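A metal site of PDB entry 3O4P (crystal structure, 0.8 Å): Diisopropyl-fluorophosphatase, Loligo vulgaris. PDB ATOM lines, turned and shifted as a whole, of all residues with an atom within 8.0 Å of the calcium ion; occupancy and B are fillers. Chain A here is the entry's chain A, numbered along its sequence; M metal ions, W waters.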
ATOM      1  N   GLY A  19      -0.575 -19.490   5.063  1.00  0.00           N
ATOM      2  CA  GLY A  19      -1.593 -19.634   4.034  1.00  0.00           C
ATOM      3  C   GLY A  19      -2.769 -18.714   4.174  1.00  0.00           C
ATOM      4  O   GLY A  19      -3.840 -19.005   3.641  1.00  0.00           O
ATOM      5  N   ALA A  20      -2.571 -17.548   4.830  1.00  0.00           N
ATOM      6  CA  ALA A  20      -3.576 -16.572   5.138  1.00  0.00           C
ATOM      7  C   ALA A  20      -4.634 -16.501   4.025  1.00  0.00           C
ATOM      8  O   ALA A  20      -4.316 -16.203   2.865  1.00  0.00           O
ATOM      9  CB  ALA A  20      -2.933 -15.202   5.308  1.00  0.00           C
ATOM     10  N   GLU A  21      -5.881 -16.672   4.428  1.00  0.00           N
ATOM     11  CA  GLU A  21      -6.978 -16.921   3.504  1.00  0.00           C
ATOM     12  C   GLU A  21      -8.275 -16.440   4.089  1.00  0.00           C
ATOM     13  O   GLU A  21      -8.385 -16.005   5.255  1.00  0.00           O
ATOM     14  CB  GLU A  21      -7.066 -18.436   3.160  1.00  0.00           C
ATOM     15  CG  GLU A  21      -6.528 -18.814   1.788  1.00  0.00           C
ATOM     16  CD  GLU A  21      -7.492 -18.553   0.676  1.00  0.00           C
ATOM     17  OE1 GLU A  21      -8.378 -17.644   0.821  1.00  0.00           O
ATOM     18  OE2 GLU A  21      -7.380 -19.278  -0.338  1.00  0.00           O
ATOM     19  N   GLY A  22      -9.326 -16.518   3.263  1.00  0.00           N
ATOM     20  CA  GLY A  22     -10.686 -16.338   3.666  1.00  0.00           C
ATOM     21  C   GLY A  22     -10.987 -15.136   4.544  1.00  0.00           C
ATOM     22  O   GLY A  22     -11.722 -15.259   5.527  1.00  0.00           O
ATOM     23  N   PRO A  36      -5.086 -21.891   6.751  1.00  0.00           N
ATOM     24  CA  PRO A  36      -5.271 -23.269   6.363  1.00  0.00           C
ATOM     25  C   PRO A  36      -4.038 -24.093   6.556  1.00  0.00           C
ATOM     26  O   PRO A  36      -4.175 -25.330   6.732  1.00  0.00           O
ATOM     27  CB  PRO A  36      -5.612 -23.198   4.860  1.00  0.00           C
ATOM     28  CG  PRO A  36      -5.270 -21.782   4.450  1.00  0.00           C
ATOM     29  CD  PRO A  36      -5.464 -20.959   5.682  1.00  0.00           C
ATOM     30  N   ALA A  74     -10.040 -22.696   4.590  1.00  0.00           N
ATOM     31  CA  ALA A  74      -9.477 -21.917   3.492  1.00  0.00           C
ATOM     32  C   ALA A  74     -10.338 -20.769   2.979  1.00  0.00           C
ATOM     33  O   ALA A  74      -9.784 -19.901   2.302  1.00  0.00           O
ATOM     34  CB  ALA A  74      -9.033 -22.789   2.342  1.00  0.00           C
ATOM     35  N   GLY A  75     -11.635 -20.749   3.239  1.00  0.00           N
ATOM     36  CA  GLY A  75     -12.475 -19.712   2.687  1.00  0.00           C
ATOM     37  C   GLY A  75     -13.704 -19.525   3.537  1.00  0.00           C
ATOM     38  O   GLY A  75     -14.161 -20.479   4.185  1.00  0.00           O
ATOM     39  N   MET A  90     -10.435 -27.747   3.272  1.00  0.00           N
ATOM     40  CA  MET A  90      -9.902 -28.676   2.305  1.00  0.00           C
ATOM     41  C   MET A  90      -9.845 -30.126   2.788  1.00  0.00           C
ATOM     42  O   MET A  90      -9.725 -31.022   1.971  1.00  0.00           O
ATOM     43  CB  MET A  90      -8.487 -28.247   1.861  1.00  0.00           C
ATOM     44  CG  MET A  90      -8.466 -26.933   1.122  1.00  0.00           C
ATOM     45  SD  MET A  90      -8.928 -27.111  -0.639  1.00  0.00           S
ATOM     46  CE  MET A  90      -7.401 -27.820  -1.284  1.00  0.00           C
ATOM     47  N   CYS A 119     -13.154 -28.469   0.368  1.00  0.00           N
ATOM     48  CA  CYS A 119     -13.563 -27.205  -0.225  1.00  0.00           C
ATOM     49  C   CYS A 119     -12.545 -26.101   0.040  1.00  0.00           C
ATOM     50  O   CYS A 119     -11.759 -26.166   0.984  1.00  0.00           O
ATOM     51  CB  CYS A 119     -14.917 -26.826   0.300  1.00  0.00           C
ATOM     52  SG  CYS A 119     -16.223 -28.001  -0.159  1.00  0.00           S
ATOM     53  N   ASN A 120     -12.581 -25.085  -0.842  1.00  0.00           N
ATOM     54  CA  ASN A 120     -11.635 -23.978  -0.730  1.00  0.00           C
ATOM     55  C   ASN A 120     -12.257 -22.613  -0.545  1.00  0.00           C
ATOM     56  O   ASN A 120     -11.763 -21.833   0.272  1.00  0.00           O
ATOM     57  CB  ASN A 120     -10.626 -23.973  -1.903  1.00  0.00           C
ATOM     58  CG  ASN A 120      -9.425 -23.073  -1.622  1.00  0.00           C
ATOM     59  OD1 ASN A 120      -9.469 -21.856  -1.815  1.00  0.00           O
ATOM     60  ND2 ASN A 120      -8.344 -23.660  -1.097  1.00  0.00           N
ATOM     61  N   ASP A 121     -13.309 -22.283  -1.305  1.00  0.00           N
ATOM     62  CA  ASP A 121     -13.952 -20.988  -1.125  1.00  0.00           C
ATOM     63  C   ASP A 121     -15.435 -21.134  -1.350  1.00  0.00           C
ATOM     64  O   ASP A 121     -15.935 -22.167  -1.833  1.00  0.00           O
ATOM     65  CB  ASP A 121     -13.286 -19.906  -2.005  1.00  0.00           C
ATOM     66  CG  ASP A 121     -13.335 -18.502  -1.408  1.00  0.00           C
ATOM     67  OD1 ASP A 121     -14.014 -18.277  -0.375  1.00  0.00           O
ATOM     68  OD2 ASP A 121     -12.660 -17.604  -2.000  1.00  0.00           O
ATOM     69  N   CYS A 122     -16.178 -20.087  -0.986  1.00  0.00           N
ATOM     70  CA  CYS A 122     -17.621 -20.128  -1.109  1.00  0.00           C
ATOM     71  C   CYS A 122     -18.171 -18.705  -1.268  1.00  0.00           C
ATOM     72  O   CYS A 122     -17.525 -17.725  -0.881  1.00  0.00           O
ATOM     73  CB  CYS A 122     -18.284 -20.938   0.013  1.00  0.00           C
ATOM     74  SG  CYS A 122     -17.982 -20.319   1.686  1.00  0.00           S
ATOM     75  N   THR A 133     -16.489 -24.021  -4.032  1.00  0.00           N
ATOM     76  CA  THR A 133     -15.492 -24.728  -4.803  1.00  0.00           C
ATOM     77  C   THR A 133     -14.868 -25.815  -3.980  1.00  0.00           C
ATOM     78  O   THR A 133     -14.585 -25.663  -2.791  1.00  0.00           O
ATOM     79  CB  THR A 133     -14.422 -23.794  -5.334  1.00  0.00           C
ATOM     80  OG1 THR A 133     -13.784 -23.173  -4.217  1.00  0.00           O
ATOM     81  CG2 THR A 133     -15.009 -22.780  -6.289  1.00  0.00           C
ATOM     82  N   PRO A 135     -11.718 -28.114  -4.632  1.00  0.00           N
ATOM     83  CA  PRO A 135     -10.563 -28.550  -5.383  1.00  0.00           C
ATOM     84  C   PRO A 135      -9.823 -29.741  -4.762  1.00  0.00           C
ATOM     85  O   PRO A 135      -8.937 -30.299  -5.435  1.00  0.00           O
ATOM     86  CB  PRO A 135      -9.661 -27.316  -5.431  1.00  0.00           C
ATOM     87  CG  PRO A 135      -9.954 -26.611  -4.112  1.00  0.00           C
ATOM     88  CD  PRO A 135     -11.433 -26.839  -3.900  1.00  0.00           C
ATOM     89  N   PHE A 173      -8.485 -27.486 -10.026  1.00  0.00           N
ATOM     90  CA  PHE A 173      -8.334 -26.545  -8.912  1.00  0.00           C
ATOM     91  C   PHE A 173      -9.268 -25.351  -9.004  1.00  0.00           C
ATOM     92  O   PHE A 173      -8.884 -24.184  -9.097  1.00  0.00           O
ATOM     93  CB  PHE A 173      -6.865 -26.104  -8.646  1.00  0.00           C
ATOM     94  CG  PHE A 173      -6.657 -25.909  -7.167  1.00  0.00           C
ATOM     95  CD1 PHE A 173      -6.984 -24.731  -6.527  1.00  0.00           C
ATOM     96  CD2 PHE A 173      -6.168 -26.941  -6.381  1.00  0.00           C
ATOM     97  CE1 PHE A 173      -6.804 -24.580  -5.174  1.00  0.00           C
ATOM     98  CE2 PHE A 173      -5.989 -26.791  -5.037  1.00  0.00           C
ATOM     99  CZ  PHE A 173      -6.332 -25.617  -4.415  1.00  0.00           C
ATOM    100  N   PRO A 174     -10.591 -25.630  -8.921  1.00  0.00           N
ATOM    101  CA  PRO A 174     -11.546 -24.534  -8.745  1.00  0.00           C
ATOM    102  C   PRO A 174     -11.248 -23.832  -7.388  1.00  0.00           C
ATOM    103  O   PRO A 174     -10.965 -24.504  -6.408  1.00  0.00           O
ATOM    104  CB  PRO A 174     -12.900 -25.250  -8.742  1.00  0.00           C
ATOM    105  CG  PRO A 174     -12.573 -26.628  -8.144  1.00  0.00           C
ATOM    106  CD  PRO A 174     -11.222 -26.928  -8.712  1.00  0.00           C
ATOM    107  N   ASN A 175     -11.340 -22.494  -7.398  1.00  0.00           N
ATOM    108  CA  ASN A 175     -10.739 -21.737  -6.312  1.00  0.00           C
ATOM    109  C   ASN A 175     -11.680 -20.642  -5.865  1.00  0.00           C
ATOM    110  O   ASN A 175     -12.705 -20.895  -5.204  1.00  0.00           O
ATOM    111  CB  ASN A 175      -9.330 -21.330  -6.673  1.00  0.00           C
ATOM    112  CG  ASN A 175      -8.505 -20.976  -5.457  1.00  0.00           C
ATOM    113  OD1 ASN A 175      -9.099 -20.673  -4.418  1.00  0.00           O
ATOM    114  ND2 ASN A 175      -7.202 -21.029  -5.565  1.00  0.00           N
ATOM    115  N   GLY A 176     -11.464 -19.372  -6.264  1.00  0.00           N
ATOM    116  CA  GLY A 176     -12.415 -18.347  -5.964  1.00  0.00           C
ATOM    117  C   GLY A 176     -13.738 -18.553  -6.691  1.00  0.00           C
ATOM    118  O   GLY A 176     -13.843 -19.264  -7.709  1.00  0.00           O
ATOM    119  N   ILE A 177     -14.753 -17.897  -6.147  1.00  0.00           N
ATOM    120  CA  ILE A 177     -16.117 -18.017  -6.650  1.00  0.00           C
ATOM    121  C   ILE A 177     -16.856 -16.757  -6.255  1.00  0.00           C
ATOM    122  O   ILE A 177     -16.607 -16.186  -5.179  1.00  0.00           O
ATOM    123  CB  ILE A 177     -16.748 -19.326  -6.128  1.00  0.00           C
ATOM    124  CG1 ILE A 177     -18.116 -19.623  -6.754  1.00  0.00           C
ATOM    125  CG2 ILE A 177     -16.768 -19.411  -4.610  1.00  0.00           C
ATOM    126  CD1 ILE A 177     -18.501 -21.102  -6.619  1.00  0.00           C
ATOM    127  N   ALA A 193     -13.100 -19.374 -10.488  1.00  0.00           N
ATOM    128  CA  ALA A 193     -11.708 -19.409 -10.881  1.00  0.00           C
ATOM    129  C   ALA A 193     -11.210 -20.832 -11.008  1.00  0.00           C
ATOM    130  O   ALA A 193     -11.494 -21.677 -10.133  1.00  0.00           O
ATOM    131  CB  ALA A 193     -10.865 -18.695  -9.822  1.00  0.00           C
ATOM    132  N   THR A 195      -7.567 -22.244 -11.049  1.00  0.00           N
ATOM    133  CA  THR A 195      -6.296 -21.545 -10.820  1.00  0.00           C
ATOM    134  C   THR A 195      -5.248 -21.777 -11.898  1.00  0.00           C
ATOM    135  O   THR A 195      -4.867 -20.806 -12.588  1.00  0.00           O
ATOM    136  CB  THR A 195      -5.771 -21.821  -9.401  1.00  0.00           C
ATOM    137  OG1 THR A 195      -6.752 -21.363  -8.461  1.00  0.00           O
ATOM    138  CG2 THR A 195      -4.440 -21.180  -9.157  1.00  0.00           C
ATOM    139  N   ALA A 228      -5.701 -17.317 -10.795  1.00  0.00           N
ATOM    140  CA  ALA A 228      -6.737 -16.699  -9.986  1.00  0.00           C
ATOM    141  C   ALA A 228      -7.004 -17.522  -8.721  1.00  0.00           C
ATOM    142  O   ALA A 228      -7.214 -18.743  -8.789  1.00  0.00           O
ATOM    143  CB  ALA A 228      -8.047 -16.627 -10.775  1.00  0.00           C
ATOM    144  N   ASP A 229      -7.055 -16.811  -7.603  1.00  0.00           N
ATOM    145  CA  ASP A 229      -7.361 -17.381  -6.293  1.00  0.00           C
ATOM    146  C   ASP A 229      -8.704 -16.796  -5.867  1.00  0.00           C
ATOM    147  O   ASP A 229      -9.728 -17.199  -6.411  1.00  0.00           O
ATOM    148  CB  ASP A 229      -6.176 -17.219  -5.356  1.00  0.00           C
ATOM    149  CG  ASP A 229      -6.332 -17.913  -4.019  1.00  0.00           C
ATOM    150  OD1 ASP A 229      -7.507 -18.242  -3.690  1.00  0.00           O
ATOM    151  OD2 ASP A 229      -5.319 -18.108  -3.310  1.00  0.00           O
ATOM    152  N   GLY A 230      -8.735 -15.806  -4.984  1.00  0.00           N
ATOM    153  CA  GLY A 230      -9.975 -15.277  -4.489  1.00  0.00           C
ATOM    154  C   GLY A 230     -10.519 -14.106  -5.274  1.00  0.00           C
ATOM    155  O   GLY A 230      -9.789 -13.407  -5.976  1.00  0.00           O
ATOM    156  N   MET A 231     -11.806 -13.845  -5.115  1.00  0.00           N
ATOM    157  CA  MET A 231     -12.463 -12.802  -5.882  1.00  0.00           C
ATOM    158  C   MET A 231     -13.624 -12.186  -5.127  1.00  0.00           C
ATOM    159  O   MET A 231     -14.235 -12.818  -4.241  1.00  0.00           O
ATOM    160  CB  MET A 231     -12.968 -13.343  -7.230  1.00  0.00           C
ATOM    161  CG  MET A 231     -14.002 -14.389  -7.072  1.00  0.00           C
ATOM    162  SD  MET A 231     -14.641 -15.072  -8.640  1.00  0.00           S
ATOM    163  CE  MET A 231     -13.101 -15.641  -9.323  1.00  0.00           C
ATOM    164  N   TRP A 244      -2.573 -15.015  -7.943  1.00  0.00           N
ATOM    165  CA  TRP A 244      -1.514 -15.517  -7.106  1.00  0.00           C
ATOM    166  C   TRP A 244      -0.312 -15.856  -7.987  1.00  0.00           C
ATOM    167  O   TRP A 244      -0.429 -16.634  -8.941  1.00  0.00           O
ATOM    168  CB  TRP A 244      -2.024 -16.781  -6.369  1.00  0.00           C
ATOM    169  CG  TRP A 244      -1.176 -17.339  -5.282  1.00  0.00           C
ATOM    170  CD1 TRP A 244      -1.495 -17.301  -3.974  1.00  0.00           C
ATOM    171  CD2 TRP A 244      -0.041 -18.195  -5.389  1.00  0.00           C
ATOM    172  NE1 TRP A 244      -0.641 -18.042  -3.224  1.00  0.00           N
ATOM    173  CE2 TRP A 244       0.278 -18.652  -4.080  1.00  0.00           C
ATOM    174  CE3 TRP A 244       0.748 -18.700  -6.425  1.00  0.00           C
ATOM    175  CZ2 TRP A 244       1.264 -19.562  -3.803  1.00  0.00           C
ATOM    176  CZ3 TRP A 244       1.751 -19.620  -6.149  1.00  0.00           C
ATOM    177  CH2 TRP A 244       1.993 -20.045  -4.862  1.00  0.00           C
ATOM    178  N   SER A 271      -3.715 -13.767  -2.375  1.00  0.00           N
ATOM    179  CA  SER A 271      -4.542 -14.960  -2.298  1.00  0.00           C
ATOM    180  C   SER A 271      -6.012 -14.635  -2.250  1.00  0.00           C
ATOM    181  O   SER A 271      -6.796 -15.078  -3.094  1.00  0.00           O
ATOM    182  CB  SER A 271      -4.144 -15.806  -1.094  1.00  0.00           C
ATOM    183  OG  SER A 271      -5.078 -16.798  -0.849  1.00  0.00           O
ATOM    184  N   ASN A 272      -6.452 -13.816  -1.330  1.00  0.00           N
ATOM    185  CA  ASN A 272      -7.873 -13.595  -1.204  1.00  0.00           C
ATOM    186  C   ASN A 272      -8.128 -12.182  -0.703  1.00  0.00           C
ATOM    187  O   ASN A 272      -7.199 -11.476  -0.280  1.00  0.00           O
ATOM    188  CB  ASN A 272      -8.546 -14.700  -0.362  1.00  0.00           C
ATOM    189  CG  ASN A 272      -9.956 -14.998  -0.802  1.00  0.00           C
ATOM    190  OD1 ASN A 272     -10.622 -14.182  -1.437  1.00  0.00           O
ATOM    191  ND2 ASN A 272     -10.396 -16.228  -0.528  1.00  0.00           N
ATOM    192  N   THR A 285      -5.162 -10.941   1.676  1.00  0.00           N
ATOM    193  CA  THR A 285      -4.250 -11.903   2.236  1.00  0.00           C
ATOM    194  C   THR A 285      -3.217 -12.277   1.176  1.00  0.00           C
ATOM    195  O   THR A 285      -3.514 -12.221  -0.020  1.00  0.00           O
ATOM    196  CB  THR A 285      -4.993 -13.145   2.749  1.00  0.00           C
ATOM    197  OG1 THR A 285      -5.520 -13.877   1.663  1.00  0.00           O
ATOM    198  CG2 THR A 285      -6.054 -12.822   3.735  1.00  0.00           C
ATOM    199  N   HIS A 287       0.595 -14.797   0.370  1.00  0.00           N
ATOM    200  CA  HIS A 287       1.371 -15.946   0.732  1.00  0.00           C
ATOM    201  C   HIS A 287       2.872 -15.814   0.512  1.00  0.00           C
ATOM    202  O   HIS A 287       3.615 -16.755   0.668  1.00  0.00           O
ATOM    203  CB  HIS A 287       0.859 -17.194   0.047  1.00  0.00           C
ATOM    204  CG  HIS A 287      -0.587 -17.523   0.380  1.00  0.00           C
ATOM    205  ND1 HIS A 287      -1.269 -18.449  -0.347  1.00  0.00           N
ATOM    206  CD2 HIS A 287      -1.391 -17.008   1.316  1.00  0.00           C
ATOM    207  CE1 HIS A 287      -2.480 -18.465   0.166  1.00  0.00           C
ATOM    208  NE2 HIS A 287      -2.599 -17.618   1.176  1.00  0.00           N
HETATM  209 CA    CA M   1      -8.659 -19.718  -2.260  1.00  0.00          CA
HETATM  210  O   HOH W   1     -10.336 -19.492  -0.459  1.00  0.00           O
HETATM  211  O   HOH W   2      -6.373 -20.659  -2.738  1.00  0.00           O
HETATM  212  O   HOH W   3     -10.369 -18.405  -3.179  1.00  0.00           O
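O of Ala 193 sits at hydrogen-bond distance from N of Asn 175, 2.9 Å away. OD2 of Asp 229 is in hydrogen-bond range of OG of Ser 271 (2.8 Å). The side-chain carboxylate (OE1) of Glu 21 is in hydrogen-bond range of the side-chain amide nitrogen (ND2) of Asn 272, at 2.8 Å. The side-chain hydroxyl (OG) of Ser 271 lies close to the side-chain carboxylate (OE2) of Glu 21, 3.4 Å away. The backbone carbonyl oxygen (O) of Asn 175 is in hydrogen-bond range of the side-chain hydroxyl (OG1) of Thr 133 (2.7 Å). The side-chain amide nitrogen (ND2) of Asn 175 is in hydrogen-bond range of the side-chain hydroxyl (OG1) of Thr 195 (2.9 Å). N of Gly 75 sits at hydrogen-bond distance from O of Asn 120. The side-chain amide nitrogen (ND2) of Asn 120 is in hydrogen-bond range of the side-chain sulfur (SD) of Met 90 (3.5 Å).
Within 4 Å of the calcium ion: Glu 21, Asn 120, Asn 175 and Asp 229. The nearest printed residue that does not touch the calcium ion is Asn 272 (4.3 Å).
The calcium ion is bound by OD1 of Asn 120 (2.3 Å), water W3 (2.3 Å), OE2 of Glu 21 (2.4 Å), OD1 of Asp 229 (2.4 Å), OD1 of Asn 175 (2.4 Å), water W1 (2.5 Å) and water W2 (2.5 Å). The calcium ion has seven donor atoms within binding distance.
Water W2 lies within hydrogen-bond range of OD2 of Asp 229 (2.8 Å) and ND2 of Asn 175 (3.0 Å). Water W3 lies within hydrogen-bond range of the side-chain carboxylate of Asp 121, the backbone NH of Gly 176 and the side-chain amide nitrogen of Asn 272.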
